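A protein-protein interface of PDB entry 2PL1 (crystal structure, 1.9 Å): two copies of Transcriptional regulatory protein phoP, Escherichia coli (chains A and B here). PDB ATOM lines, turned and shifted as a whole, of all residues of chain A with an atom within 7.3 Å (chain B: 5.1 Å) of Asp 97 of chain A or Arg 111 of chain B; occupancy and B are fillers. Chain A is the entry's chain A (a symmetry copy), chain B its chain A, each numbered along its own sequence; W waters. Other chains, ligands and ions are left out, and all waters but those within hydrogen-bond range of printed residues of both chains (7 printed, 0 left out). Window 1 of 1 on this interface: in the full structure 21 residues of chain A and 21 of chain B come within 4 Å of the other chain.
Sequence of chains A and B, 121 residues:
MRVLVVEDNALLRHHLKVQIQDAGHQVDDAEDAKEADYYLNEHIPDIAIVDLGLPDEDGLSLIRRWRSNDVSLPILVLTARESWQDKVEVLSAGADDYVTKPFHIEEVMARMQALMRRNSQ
OE2 of Glu 107 of chain B lies within salt-bridge range of NE of Arg 111 of chain B (2.8 Å).
O of Ile 75 of chain A lies within hydrogen-bond range of N of Asp 97 of chain A, at 3.4 Å.
N of Val 77 of chain A lies within hydrogen-bond range of O of Asp 97 of chain A.
O of Val 88 of chain A lies within hydrogen-bond range of OG of Ser 92 of chain A (2.6 Å).
The side-chain carboxylate (OD2) of Asp 97 of chain A is in salt-bridge range of the guanidinium group (NH1) of Arg 111 of chain A.
NE of Arg 111 of chain A is in salt-bridge range of OE2 of Glu 107 of chain A, 2.8 Å away.
NH1 of Arg 111 of chain A lies within salt-bridge range of OD1 of Asp 97 of chain B (2.9 Å).
The guanidinium group (NH1) of Arg 111 of chain B is in salt-bridge range of the side-chain carboxylate (OD1) of Asp 97 of chain A, 2.9 Å away.
The backbone carbonyl oxygen (O) of Tyr 98 of chain A lies within hydrogen-bond range of the guanidinium group (NH2) of Arg 111 of chain B (3.1 Å).
Asp 97 of chain A touches just one residue of chain B: Arg 111 (2.9 Å).
Arg 111 of chain B touches just these residues of chain A: Leu 91, Asp 97 and Tyr 98.
No residue of chain A comes within 4 Å of Ala 110 of chain B.
Of the printed residues of chain B, Leu 91 of chain A touches Arg 111.
Of the printed residues of chain A, Asp 97 of chain B touches Arg 111.
Printed residues of chain A within 4 Å of Glu 107 of chain B: Lys 87 (3.6 Å) and Val 88 (3.7 Å).
Met 112 of chain A touches none of the printed residues of chain B.
Leu 115 of chain A touches none of the printed residues of chain B.
The nearest residue of chain A that does not touch Arg 111 of chain B is Arg 111 of chain A (4.5 Å).
The nearest printed residue of chain B that does not touch Leu 91 of chain A is Ala 110 of chain B (4.2 Å).
Among the printed residues, pairs that only touch across the chains: Lys 87 of chain A with Glu 107 of chain B (3.6 Å), Val 88 of chain A with Glu 107 of chain B (3.7 Å) and Leu 91 of chain A with Arg 111 of chain B (3.6 Å).
Of the 13 printed residues of chain B, 3 touch a printed residue of chain A.
Of the 26 printed residues of chain A, 6 touch a printed residue of chain B.
Hydrophobic or aromatic side chains of chain A within 4 Å of the printed part of chain B: Val 88, Leu 91 and Tyr 98.
Among the printed residues, 6 pairs touch across the chains.
Asp 97 of chain A touches Arg 111 of chain B, and with the chains exchanged Arg 111 of chain A touches Asp 97 of chain B.
Positions printed for both chains: 76, 96, 97, 99, 107, 108, 110, 111, 112, 114 and 115.
Of the 6 pairs that touch across the chains among the printed residues, 2 have their exchanged pair printed and touching as well.
Water W1 bridges the side-chain carboxylate (OE1) of Glu 107 of chain B (2.6 Å) and the side-chain amino group (NZ) of Lys 87 of chain A (2.8 Å).
Water W2 bridges OD1 of Asp 96 of chain A and O of Ala 114 of chain B.
Water W5 bridges the side-chain hydroxyl (OG) of Ser 92 of chain A (2.8 Å) and the side-chain amide nitrogen (NE2) of Gln 113 of chain B (3.0 Å).
Water W6 lies within hydrogen-bond range of NH2 of Arg 111 of chain A (3.2 Å), OD1 of Asp 97 of chain B (3.3 Å) and NH2 of Arg 111 of chain B (3.3 Å).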
ATOM      1  N   VAL A  50      -4.685 -10.869 -31.942  1.00  0.00           N
ATOM      2  CA  VAL A  50      -3.707 -10.257 -32.828  1.00  0.00           C
ATOM      3  C   VAL A  50      -2.276 -10.760 -32.727  1.00  0.00           C
ATOM      4  O   VAL A  50      -1.684 -10.821 -31.646  1.00  0.00           O
ATOM      5  CB  VAL A  50      -3.714  -8.723 -32.622  1.00  0.00           C
ATOM      6  CG1 VAL A  50      -2.711  -8.046 -33.550  1.00  0.00           C
ATOM      7  CG2 VAL A  50      -5.115  -8.192 -32.860  1.00  0.00           C
ATOM      8  N   ILE A  63      -2.330  -2.078 -33.246  1.00  0.00           N
ATOM      9  CA  ILE A  63      -3.008  -1.848 -31.975  1.00  0.00           C
ATOM     10  C   ILE A  63      -2.986  -0.367 -31.590  1.00  0.00           C
ATOM     11  O   ILE A  63      -4.009   0.193 -31.202  1.00  0.00           O
ATOM     12  CB  ILE A  63      -2.366  -2.696 -30.856  1.00  0.00           C
ATOM     13  CG1 ILE A  63      -2.606  -4.180 -31.144  1.00  0.00           C
ATOM     14  CG2 ILE A  63      -2.948  -2.310 -29.499  1.00  0.00           C
ATOM     15  CD1 ILE A  63      -1.872  -5.123 -30.199  1.00  0.00           C
ATOM     16  N   PRO A  74     -11.819  -5.523 -26.790  1.00  0.00           N
ATOM     17  CA  PRO A  74     -10.743  -6.282 -26.143  1.00  0.00           C
ATOM     18  C   PRO A  74      -9.799  -6.904 -27.171  1.00  0.00           C
ATOM     19  O   PRO A  74     -10.245  -7.469 -28.176  1.00  0.00           O
ATOM     20  CB  PRO A  74     -11.493  -7.343 -25.344  1.00  0.00           C
ATOM     21  CG  PRO A  74     -12.820  -6.681 -25.051  1.00  0.00           C
ATOM     22  CD  PRO A  74     -13.141  -6.021 -26.368  1.00  0.00           C
ATOM     23  N   ILE A  75      -8.497  -6.799 -26.918  1.00  0.00           N
ATOM     24  CA  ILE A  75      -7.504  -7.365 -27.818  1.00  0.00           C
ATOM     25  C   ILE A  75      -6.548  -8.294 -27.077  1.00  0.00           C
ATOM     26  O   ILE A  75      -5.912  -7.896 -26.097  1.00  0.00           O
ATOM     27  CB  ILE A  75      -6.665  -6.265 -28.509  1.00  0.00           C
ATOM     28  CG1 ILE A  75      -7.562  -5.396 -29.394  1.00  0.00           C
ATOM     29  CG2 ILE A  75      -5.550  -6.905 -29.346  1.00  0.00           C
ATOM     30  CD1 ILE A  75      -6.835  -4.240 -30.048  1.00  0.00           C
ATOM     31  N   LEU A  76      -6.463  -9.536 -27.541  1.00  0.00           N
ATOM     32  CA  LEU A  76      -5.559 -10.507 -26.945  1.00  0.00           C
ATOM     33  C   LEU A  76      -4.480 -10.787 -27.979  1.00  0.00           C
ATOM     34  O   LEU A  76      -4.775 -11.197 -29.103  1.00  0.00           O
ATOM     35  CB  LEU A  76      -6.298 -11.803 -26.578  1.00  0.00           C
ATOM     36  CG  LEU A  76      -5.454 -12.943 -25.980  1.00  0.00           C
ATOM     37  CD1 LEU A  76      -6.333 -13.849 -25.134  1.00  0.00           C
ATOM     38  CD2 LEU A  76      -4.780 -13.742 -27.092  1.00  0.00           C
ATOM     39  N   VAL A  77      -3.233 -10.532 -27.605  1.00  0.00           N
ATOM     40  CA  VAL A  77      -2.110 -10.763 -28.505  1.00  0.00           C
ATOM     41  C   VAL A  77      -1.570 -12.182 -28.329  1.00  0.00           C
ATOM     42  O   VAL A  77      -1.418 -12.665 -27.209  1.00  0.00           O
ATOM     43  CB  VAL A  77      -0.990  -9.732 -28.242  1.00  0.00           C
ATOM     44  CG1 VAL A  77       0.288 -10.115 -28.996  1.00  0.00           C
ATOM     45  CG2 VAL A  77      -1.462  -8.354 -28.678  1.00  0.00           C
ATOM     46  N   LEU A  78      -1.313 -12.849 -29.452  1.00  0.00           N
ATOM     47  CA  LEU A  78      -0.789 -14.214 -29.475  1.00  0.00           C
ATOM     48  C   LEU A  78       0.396 -14.117 -30.419  1.00  0.00           C
ATOM     49  O   LEU A  78       0.224 -13.985 -31.634  1.00  0.00           O
ATOM     50  CB  LEU A  78      -1.847 -15.175 -30.026  1.00  0.00           C
ATOM     51  CG  LEU A  78      -1.467 -16.655 -30.134  1.00  0.00           C
ATOM     52  CD1 LEU A  78      -1.032 -17.195 -28.773  1.00  0.00           C
ATOM     53  CD2 LEU A  78      -2.671 -17.433 -30.665  1.00  0.00           C
ATOM     54  N   LYS A  87       6.048  -7.559 -23.863  1.00  0.00           N
ATOM     55  CA  LYS A  87       4.749  -7.745 -23.227  1.00  0.00           C
ATOM     56  C   LYS A  87       4.312  -6.433 -22.582  1.00  0.00           C
ATOM     57  O   LYS A  87       3.162  -6.007 -22.715  1.00  0.00           O
ATOM     58  CB  LYS A  87       4.830  -8.850 -22.165  1.00  0.00           C
ATOM     59  CG  LYS A  87       5.114 -10.234 -22.740  1.00  0.00           C
ATOM     60  CD  LYS A  87       5.074 -11.321 -21.670  1.00  0.00           C
ATOM     61  CE  LYS A  87       5.477 -12.672 -22.255  1.00  0.00           C
ATOM     62  NZ  LYS A  87       5.353 -13.773 -21.255  1.00  0.00           N
ATOM     63  N   VAL A  88       5.245  -5.785 -21.890  1.00  0.00           N
ATOM     64  CA  VAL A  88       4.960  -4.521 -21.225  1.00  0.00           C
ATOM     65  C   VAL A  88       4.598  -3.430 -22.225  1.00  0.00           C
ATOM     66  O   VAL A  88       3.632  -2.693 -22.033  1.00  0.00           O
ATOM     67  CB  VAL A  88       6.171  -4.054 -20.388  1.00  0.00           C
ATOM     68  CG1 VAL A  88       5.985  -2.598 -19.954  1.00  0.00           C
ATOM     69  CG2 VAL A  88       6.327  -4.953 -19.169  1.00  0.00           C
ATOM     70  N   VAL A  90       3.504  -3.771 -25.375  1.00  0.00           N
ATOM     71  CA  VAL A  90       2.273  -4.095 -26.084  1.00  0.00           C
ATOM     72  C   VAL A  90       1.039  -3.918 -25.199  1.00  0.00           C
ATOM     73  O   VAL A  90       0.007  -3.408 -25.646  1.00  0.00           O
ATOM     74  CB  VAL A  90       2.344  -5.536 -26.641  1.00  0.00           C
ATOM     75  CG1 VAL A  90       1.007  -5.946 -27.229  1.00  0.00           C
ATOM     76  CG2 VAL A  90       3.439  -5.609 -27.715  1.00  0.00           C
ATOM     77  N   LEU A  91       1.143  -4.329 -23.943  1.00  0.00           N
ATOM     78  CA  LEU A  91       0.026  -4.167 -23.022  1.00  0.00           C
ATOM     79  C   LEU A  91      -0.186  -2.674 -22.773  1.00  0.00           C
ATOM     80  O   LEU A  91      -1.318  -2.201 -22.743  1.00  0.00           O
ATOM     81  CB  LEU A  91       0.312  -4.892 -21.702  1.00  0.00           C
ATOM     82  CG  LEU A  91       0.284  -6.425 -21.748  1.00  0.00           C
ATOM     83  CD1 LEU A  91       0.858  -6.994 -20.454  1.00  0.00           C
ATOM     84  CD2 LEU A  91      -1.146  -6.902 -21.963  1.00  0.00           C
ATOM     85  N   SER A  92       0.906  -1.929 -22.620  1.00  0.00           N
ATOM     86  CA  SER A  92       0.809  -0.490 -22.378  1.00  0.00           C
ATOM     87  C   SER A  92       0.217   0.231 -23.582  1.00  0.00           C
ATOM     88  O   SER A  92      -0.404   1.281 -23.445  1.00  0.00           O
ATOM     89  CB  SER A  92       2.189   0.099 -22.065  1.00  0.00           C
ATOM     90  OG  SER A  92       2.767  -0.536 -20.936  1.00  0.00           O
ATOM     91  N   GLY A  94      -2.180  -0.847 -25.330  1.00  0.00           N
ATOM     92  CA  GLY A  94      -3.613  -1.077 -25.416  1.00  0.00           C
ATOM     93  C   GLY A  94      -4.073  -2.523 -25.475  1.00  0.00           C
ATOM     94  O   GLY A  94      -5.275  -2.790 -25.447  1.00  0.00           O
ATOM     95  N   ALA A  95      -3.143  -3.469 -25.572  1.00  0.00           N
ATOM     96  CA  ALA A  95      -3.538  -4.877 -25.612  1.00  0.00           C
ATOM     97  C   ALA A  95      -4.103  -5.233 -24.238  1.00  0.00           C
ATOM     98  O   ALA A  95      -3.695  -4.659 -23.233  1.00  0.00           O
ATOM     99  CB  ALA A  95      -2.337  -5.758 -25.931  1.00  0.00           C
ATOM    100  N   ASP A  96      -5.039  -6.177 -24.200  1.00  0.00           N
ATOM    101  CA  ASP A  96      -5.656  -6.589 -22.945  1.00  0.00           C
ATOM    102  C   ASP A  96      -5.015  -7.828 -22.343  1.00  0.00           C
ATOM    103  O   ASP A  96      -5.122  -8.073 -21.143  1.00  0.00           O
ATOM    104  CB  ASP A  96      -7.148  -6.827 -23.160  1.00  0.00           C
ATOM    105  CG  ASP A  96      -7.894  -5.542 -23.407  1.00  0.00           C
ATOM    106  OD1 ASP A  96      -8.201  -4.845 -22.417  1.00  0.00           O
ATOM    107  OD2 ASP A  96      -8.145  -5.216 -24.588  1.00  0.00           O
ATOM    108  N   ASP A  97      -4.367  -8.621 -23.183  1.00  0.00           N
ATOM    109  CA  ASP A  97      -3.693  -9.818 -22.709  1.00  0.00           C
ATOM    110  C   ASP A  97      -2.620 -10.135 -23.734  1.00  0.00           C
ATOM    111  O   ASP A  97      -2.659  -9.637 -24.860  1.00  0.00           O
ATOM    112  CB  ASP A  97      -4.675 -10.985 -22.551  1.00  0.00           C
ATOM    113  CG  ASP A  97      -4.169 -12.051 -21.576  1.00  0.00           C
ATOM    114  OD1 ASP A  97      -2.962 -12.071 -21.265  1.00  0.00           O
ATOM    115  OD2 ASP A  97      -4.983 -12.879 -21.124  1.00  0.00           O
ATOM    116  N   TYR A  98      -1.665 -10.961 -23.339  1.00  0.00           N
ATOM    117  CA  TYR A  98      -0.544 -11.296 -24.199  1.00  0.00           C
ATOM    118  C   TYR A  98      -0.137 -12.737 -23.912  1.00  0.00           C
ATOM    119  O   TYR A  98       0.228 -13.073 -22.784  1.00  0.00           O
ATOM    120  CB  TYR A  98       0.566 -10.337 -23.894  1.00  0.00           C
ATOM    121  CG  TYR A  98       1.806 -10.303 -24.785  1.00  0.00           C
ATOM    122  CD1 TYR A  98       2.599 -11.436 -24.967  1.00  0.00           C
ATOM    123  CD2 TYR A  98       2.139  -9.143 -25.478  1.00  0.00           C
ATOM    124  CE1 TYR A  98       3.752 -11.385 -25.758  1.00  0.00           C
ATOM    125  CE2 TYR A  98       3.287  -9.077 -26.267  1.00  0.00           C
ATOM    126  CZ  TYR A  98       4.090 -10.199 -26.399  1.00  0.00           C
ATOM    127  OH  TYR A  98       5.233 -10.123 -27.159  1.00  0.00           O
ATOM    128  N   VAL A  99      -0.232 -13.585 -24.935  1.00  0.00           N
ATOM    129  CA  VAL A  99       0.122 -14.996 -24.818  1.00  0.00           C
ATOM    130  C   VAL A  99       1.223 -15.315 -25.825  1.00  0.00           C
ATOM    131  O   VAL A  99       1.188 -14.846 -26.963  1.00  0.00           O
ATOM    132  CB  VAL A  99      -1.100 -15.895 -25.100  1.00  0.00           C
ATOM    133  CG1 VAL A  99      -0.708 -17.374 -25.007  1.00  0.00           C
ATOM    134  CG2 VAL A  99      -2.206 -15.578 -24.110  1.00  0.00           C
ATOM    135  N   THR A 100       2.206 -16.105 -25.405  1.00  0.00           N
ATOM    136  CA  THR A 100       3.310 -16.453 -26.290  1.00  0.00           C
ATOM    137  C   THR A 100       3.122 -17.795 -26.984  1.00  0.00           C
ATOM    138  O   THR A 100       2.423 -18.677 -26.481  1.00  0.00           O
ATOM    139  CB  THR A 100       4.646 -16.509 -25.515  1.00  0.00           C
ATOM    140  OG1 THR A 100       4.529 -17.428 -24.420  1.00  0.00           O
ATOM    141  CG2 THR A 100       5.010 -15.136 -24.973  1.00  0.00           C
ATOM    142  N   GLU A 107      -5.722 -22.570 -22.931  1.00  0.00           N
ATOM    143  CA  GLU A 107      -5.439 -21.355 -22.167  1.00  0.00           C
ATOM    144  C   GLU A 107      -5.881 -20.110 -22.929  1.00  0.00           C
ATOM    145  O   GLU A 107      -6.410 -19.168 -22.339  1.00  0.00           O
ATOM    146  CB  GLU A 107      -3.949 -21.235 -21.841  1.00  0.00           C
ATOM    147  CG  GLU A 107      -3.645 -20.007 -20.984  1.00  0.00           C
ATOM    148  CD  GLU A 107      -2.162 -19.798 -20.716  1.00  0.00           C
ATOM    149  OE1 GLU A 107      -1.362 -20.732 -20.951  1.00  0.00           O
ATOM    150  OE2 GLU A 107      -1.804 -18.691 -20.255  1.00  0.00           O
ATOM    151  N   VAL A 108      -5.653 -20.102 -24.239  1.00  0.00           N
ATOM    152  CA  VAL A 108      -6.045 -18.962 -25.057  1.00  0.00           C
ATOM    153  C   VAL A 108      -7.554 -18.810 -24.973  1.00  0.00           C
ATOM    154  O   VAL A 108      -8.076 -17.707 -24.813  1.00  0.00           O
ATOM    155  CB  VAL A 108      -5.644 -19.162 -26.529  1.00  0.00           C
ATOM    156  CG1 VAL A 108      -6.195 -18.018 -27.386  1.00  0.00           C
ATOM    157  CG2 VAL A 108      -4.124 -19.232 -26.643  1.00  0.00           C
ATOM    158  N   ALA A 110      -9.526 -19.887 -22.582  1.00  0.00           N
ATOM    159  CA  ALA A 110      -9.891 -19.424 -21.244  1.00  0.00           C
ATOM    160  C   ALA A 110      -9.625 -17.926 -21.098  1.00  0.00           C
ATOM    161  O   ALA A 110     -10.371 -17.219 -20.424  1.00  0.00           O
ATOM    162  CB  ALA A 110      -9.108 -20.197 -20.185  1.00  0.00           C
ATOM    163  N   ARG A 111      -8.564 -17.437 -21.731  1.00  0.00           N
ATOM    164  CA  ARG A 111      -8.254 -16.016 -21.642  1.00  0.00           C
ATOM    165  C   ARG A 111      -9.218 -15.179 -22.469  1.00  0.00           C
ATOM    166  O   ARG A 111      -9.531 -14.046 -22.107  1.00  0.00           O
ATOM    167  CB  ARG A 111      -6.806 -15.764 -22.055  1.00  0.00           C
ATOM    168  CG  ARG A 111      -5.826 -16.235 -20.983  1.00  0.00           C
ATOM    169  CD  ARG A 111      -4.376 -16.062 -21.396  1.00  0.00           C
ATOM    170  NE  ARG A 111      -3.476 -16.454 -20.317  1.00  0.00           N
ATOM    171  CZ  ARG A 111      -3.201 -15.710 -19.249  1.00  0.00           C
ATOM    172  NH1 ARG A 111      -3.751 -14.511 -19.100  1.00  0.00           N
ATOM    173  NH2 ARG A 111      -2.377 -16.175 -18.319  1.00  0.00           N
ATOM    174  N   MET A 112      -9.696 -15.739 -23.575  1.00  0.00           N
ATOM    175  CA  MET A 112     -10.666 -15.036 -24.412  1.00  0.00           C
ATOM    176  C   MET A 112     -11.979 -14.936 -23.638  1.00  0.00           C
ATOM    177  O   MET A 112     -12.647 -13.903 -23.646  1.00  0.00           O
ATOM    178  CB  MET A 112     -10.910 -15.798 -25.720  1.00  0.00           C
ATOM    179  CG  MET A 112      -9.814 -15.643 -26.746  1.00  0.00           C
ATOM    180  SD  MET A 112     -10.264 -16.568 -28.385  1.00  0.00           S
ATOM    181  CE  MET A 112     -11.909 -15.654 -28.805  1.00  0.00           C
ATOM    182  N   ALA A 114     -12.341 -14.929 -20.428  1.00  0.00           N
ATOM    183  CA  ALA A 114     -12.188 -13.983 -19.326  1.00  0.00           C
ATOM    184  C   ALA A 114     -12.478 -12.571 -19.842  1.00  0.00           C
ATOM    185  O   ALA A 114     -13.196 -11.809 -19.201  1.00  0.00           O
ATOM    186  CB  ALA A 114     -10.775 -14.055 -18.753  1.00  0.00           C
ATOM    187  N   LEU A 115     -11.925 -12.230 -21.003  1.00  0.00           N
ATOM    188  CA  LEU A 115     -12.152 -10.908 -21.588  1.00  0.00           C
ATOM    189  C   LEU A 115     -13.620 -10.722 -21.985  1.00  0.00           C
ATOM    190  O   LEU A 115     -14.231  -9.700 -21.666  1.00  0.00           O
ATOM    191  CB  LEU A 115     -11.254 -10.698 -22.813  1.00  0.00           C
ATOM    192  CG  LEU A 115      -9.757 -10.494 -22.544  1.00  0.00           C
ATOM    193  CD1 LEU A 115      -8.974 -10.566 -23.849  1.00  0.00           C
ATOM    194  CD2 LEU A 115      -9.537  -9.151 -21.860  1.00  0.00           C
ATOM    195  N   LEU B  76      -6.337 -10.485 -10.494  1.00  0.00           N
ATOM    196  CA  LEU B  76      -5.139 -10.935 -11.185  1.00  0.00           C
ATOM    197  C   LEU B  76      -4.417 -11.874 -10.232  1.00  0.00           C
ATOM    198  O   LEU B  76      -4.076 -11.495  -9.110  1.00  0.00           O
ATOM    199  CB  LEU B  76      -4.235  -9.751 -11.558  1.00  0.00           C
ATOM    200  CG  LEU B  76      -2.903 -10.084 -12.256  1.00  0.00           C
ATOM    201  CD1 LEU B  76      -2.440  -8.896 -13.083  1.00  0.00           C
ATOM    202  CD2 LEU B  76      -1.844 -10.456 -11.221  1.00  0.00           C
ATOM    203  N   ASP B  96      -9.129 -12.919 -13.774  1.00  0.00           N
ATOM    204  CA  ASP B  96      -9.054 -12.141 -15.005  1.00  0.00           C
ATOM    205  C   ASP B  96      -7.705 -12.247 -15.695  1.00  0.00           C
ATOM    206  O   ASP B  96      -7.591 -12.007 -16.896  1.00  0.00           O
ATOM    207  CB  ASP B  96      -9.372 -10.679 -14.708  1.00  0.00           C
ATOM    208  CG  ASP B  96     -10.824 -10.477 -14.362  1.00  0.00           C
ATOM    209  OD1 ASP B  96     -11.645 -10.411 -15.301  1.00  0.00           O
ATOM    210  OD2 ASP B  96     -11.146 -10.416 -13.155  1.00  0.00           O
ATOM    211  N   ASP B  97      -6.678 -12.587 -14.931  1.00  0.00           N
ATOM    212  CA  ASP B  97      -5.348 -12.745 -15.495  1.00  0.00           C
ATOM    213  C   ASP B  97      -4.594 -13.665 -14.552  1.00  0.00           C
ATOM    214  O   ASP B  97      -5.000 -13.861 -13.406  1.00  0.00           O
ATOM    215  CB  ASP B  97      -4.640 -11.393 -15.641  1.00  0.00           C
ATOM    216  CG  ASP B  97      -3.524 -11.423 -16.688  1.00  0.00           C
ATOM    217  OD1 ASP B  97      -3.078 -12.522 -17.075  1.00  0.00           O
ATOM    218  OD2 ASP B  97      -3.086 -10.341 -17.124  1.00  0.00           O
ATOM    219  N   VAL B  99      -0.438 -14.641 -13.647  1.00  0.00           N
ATOM    220  CA  VAL B  99       0.995 -14.437 -13.844  1.00  0.00           C
ATOM    221  C   VAL B  99       1.759 -15.381 -12.921  1.00  0.00           C
ATOM    222  O   VAL B  99       1.382 -15.571 -11.765  1.00  0.00           O
ATOM    223  CB  VAL B  99       1.392 -12.980 -13.525  1.00  0.00           C
ATOM    224  CG1 VAL B  99       2.903 -12.788 -13.702  1.00  0.00           C
ATOM    225  CG2 VAL B  99       0.628 -12.033 -14.431  1.00  0.00           C
ATOM    226  N   GLU B 107       5.733  -6.116 -15.681  1.00  0.00           N
ATOM    227  CA  GLU B 107       4.665  -6.799 -16.409  1.00  0.00           C
ATOM    228  C   GLU B 107       3.393  -6.887 -15.571  1.00  0.00           C
ATOM    229  O   GLU B 107       2.289  -6.722 -16.087  1.00  0.00           O
ATOM    230  CB  GLU B 107       5.085  -8.212 -16.822  1.00  0.00           C
ATOM    231  CG  GLU B 107       4.007  -8.916 -17.643  1.00  0.00           C
ATOM    232  CD  GLU B 107       4.346 -10.356 -17.993  1.00  0.00           C
ATOM    233  OE1 GLU B 107       5.522 -10.759 -17.847  1.00  0.00           O
ATOM    234  OE2 GLU B 107       3.424 -11.082 -18.429  1.00  0.00           O
ATOM    235  N   VAL B 108       3.551  -7.155 -14.277  1.00  0.00           N
ATOM    236  CA  VAL B 108       2.400  -7.252 -13.391  1.00  0.00           C
ATOM    237  C   VAL B 108       1.696  -5.906 -13.374  1.00  0.00           C
ATOM    238  O   VAL B 108       0.470  -5.827 -13.455  1.00  0.00           O
ATOM    239  CB  VAL B 108       2.826  -7.609 -11.955  1.00  0.00           C
ATOM    240  CG1 VAL B 108       1.614  -7.562 -11.019  1.00  0.00           C
ATOM    241  CG2 VAL B 108       3.460  -8.997 -11.939  1.00  0.00           C
ATOM    242  N   MET B 109       2.494  -4.851 -13.275  1.00  0.00           N
ATOM    243  CA  MET B 109       1.995  -3.481 -13.244  1.00  0.00           C
ATOM    244  C   MET B 109       1.231  -3.196 -14.551  1.00  0.00           C
ATOM    245  O   MET B 109       0.131  -2.641 -14.534  1.00  0.00           O
ATOM    246  CB  MET B 109       3.184  -2.523 -13.097  1.00  0.00           C
ATOM    247  CG  MET B 109       2.881  -1.182 -12.459  1.00  0.00           C
ATOM    248  SD  MET B 109       2.531  -1.274 -10.551  1.00  0.00           S
ATOM    249  CE  MET B 109       4.310  -1.631  -9.904  1.00  0.00           C
ATOM    250  N   ALA B 110       1.816  -3.576 -15.682  1.00  0.00           N
ATOM    251  CA  ALA B 110       1.169  -3.355 -16.975  1.00  0.00           C
ATOM    252  C   ALA B 110      -0.130  -4.155 -17.074  1.00  0.00           C
ATOM    253  O   ALA B 110      -1.103  -3.699 -17.671  1.00  0.00           O
ATOM    254  CB  ALA B 110       2.110  -3.748 -18.112  1.00  0.00           C
ATOM    255  N   ARG B 111      -0.151  -5.346 -16.488  1.00  0.00           N
ATOM    256  CA  ARG B 111      -1.359  -6.160 -16.536  1.00  0.00           C
ATOM    257  C   ARG B 111      -2.441  -5.614 -15.618  1.00  0.00           C
ATOM    258  O   ARG B 111      -3.629  -5.731 -15.912  1.00  0.00           O
ATOM    259  CB  ARG B 111      -1.031  -7.615 -16.204  1.00  0.00           C
ATOM    260  CG  ARG B 111      -0.297  -8.302 -17.353  1.00  0.00           C
ATOM    261  CD  ARG B 111       0.105  -9.727 -17.023  1.00  0.00           C
ATOM    262  NE  ARG B 111       0.735 -10.371 -18.171  1.00  0.00           N
ATOM    263  CZ  ARG B 111       0.081 -10.858 -19.222  1.00  0.00           C
ATOM    264  NH1 ARG B 111      -1.243 -10.790 -19.287  1.00  0.00           N
ATOM    265  NH2 ARG B 111       0.760 -11.410 -20.220  1.00  0.00           N
ATOM    266  N   MET B 112      -2.030  -5.008 -14.508  1.00  0.00           N
ATOM    267  CA  MET B 112      -2.989  -4.406 -13.585  1.00  0.00           C
ATOM    268  C   MET B 112      -3.616  -3.194 -14.271  1.00  0.00           C
ATOM    269  O   MET B 112      -4.821  -2.961 -14.179  1.00  0.00           O
ATOM    270  CB  MET B 112      -2.294  -3.951 -12.297  1.00  0.00           C
ATOM    271  CG  MET B 112      -1.967  -5.067 -11.336  1.00  0.00           C
ATOM    272  SD  MET B 112      -1.176  -4.373  -9.712  1.00  0.00           S
ATOM    273  CE  MET B 112      -2.606  -3.208  -9.153  1.00  0.00           C
ATOM    274  N   GLN B 113      -2.783  -2.421 -14.959  1.00  0.00           N
ATOM    275  CA  GLN B 113      -3.254  -1.236 -15.662  1.00  0.00           C
ATOM    276  C   GLN B 113      -4.220  -1.612 -16.776  1.00  0.00           C
ATOM    277  O   GLN B 113      -5.194  -0.901 -17.021  1.00  0.00           O
ATOM    278  CB  GLN B 113      -2.065  -0.455 -16.224  1.00  0.00           C
ATOM    279  CG  GLN B 113      -1.166   0.115 -15.136  1.00  0.00           C
ATOM    280  CD  GLN B 113       0.085   0.777 -15.679  1.00  0.00           C
ATOM    281  OE1 GLN B 113       0.935   1.242 -14.913  1.00  0.00           O
ATOM    282  NE2 GLN B 113       0.208   0.826 -17.003  1.00  0.00           N
ATOM    283  N   ALA B 114      -3.955  -2.728 -17.451  1.00  0.00           N
ATOM    284  CA  ALA B 114      -4.843  -3.177 -18.519  1.00  0.00           C
ATOM    285  C   ALA B 114      -6.227  -3.456 -17.927  1.00  0.00           C
ATOM    286  O   ALA B 114      -7.239  -3.049 -18.491  1.00  0.00           O
ATOM    287  CB  ALA B 114      -4.288  -4.436 -19.181  1.00  0.00           C
ATOM    288  N   LEU B 115      -6.267  -4.145 -16.790  1.00  0.00           N
ATOM    289  CA  LEU B 115      -7.541  -4.452 -16.138  1.00  0.00           C
ATOM    290  C   LEU B 115      -8.232  -3.178 -15.644  1.00  0.00           C
ATOM    291  O   LEU B 115      -9.425  -2.979 -15.881  1.00  0.00           O
ATOM    292  CB  LEU B 115      -7.327  -5.414 -14.963  1.00  0.00           C
ATOM    293  CG  LEU B 115      -6.978  -6.866 -15.314  1.00  0.00           C
ATOM    294  CD1 LEU B 115      -6.540  -7.619 -14.064  1.00  0.00           C
ATOM    295  CD2 LEU B 115      -8.183  -7.542 -15.953  1.00  0.00           C
HETATM  296  O   HOH W   1       6.375 -13.069 -18.765  1.00  0.00           O
HETATM  297  O   HOH W   2      -6.961  -2.780 -21.211  1.00  0.00           O
HETATM  298  O   HOH W   3     -13.174 -12.280 -16.495  1.00  0.00           O
HETATM  299  O   HOH W   4      -1.076  -1.734 -19.589  1.00  0.00           O
HETATM  300  O   HOH W   5       2.740  -0.252 -18.150  1.00  0.00           O
HETATM  301  O   HOH W   6      -0.221 -13.762 -18.085  1.00  0.00           O
HETATM  302  O   HOH W   7      -0.692 -14.299 -20.486  1.00  0.00           O
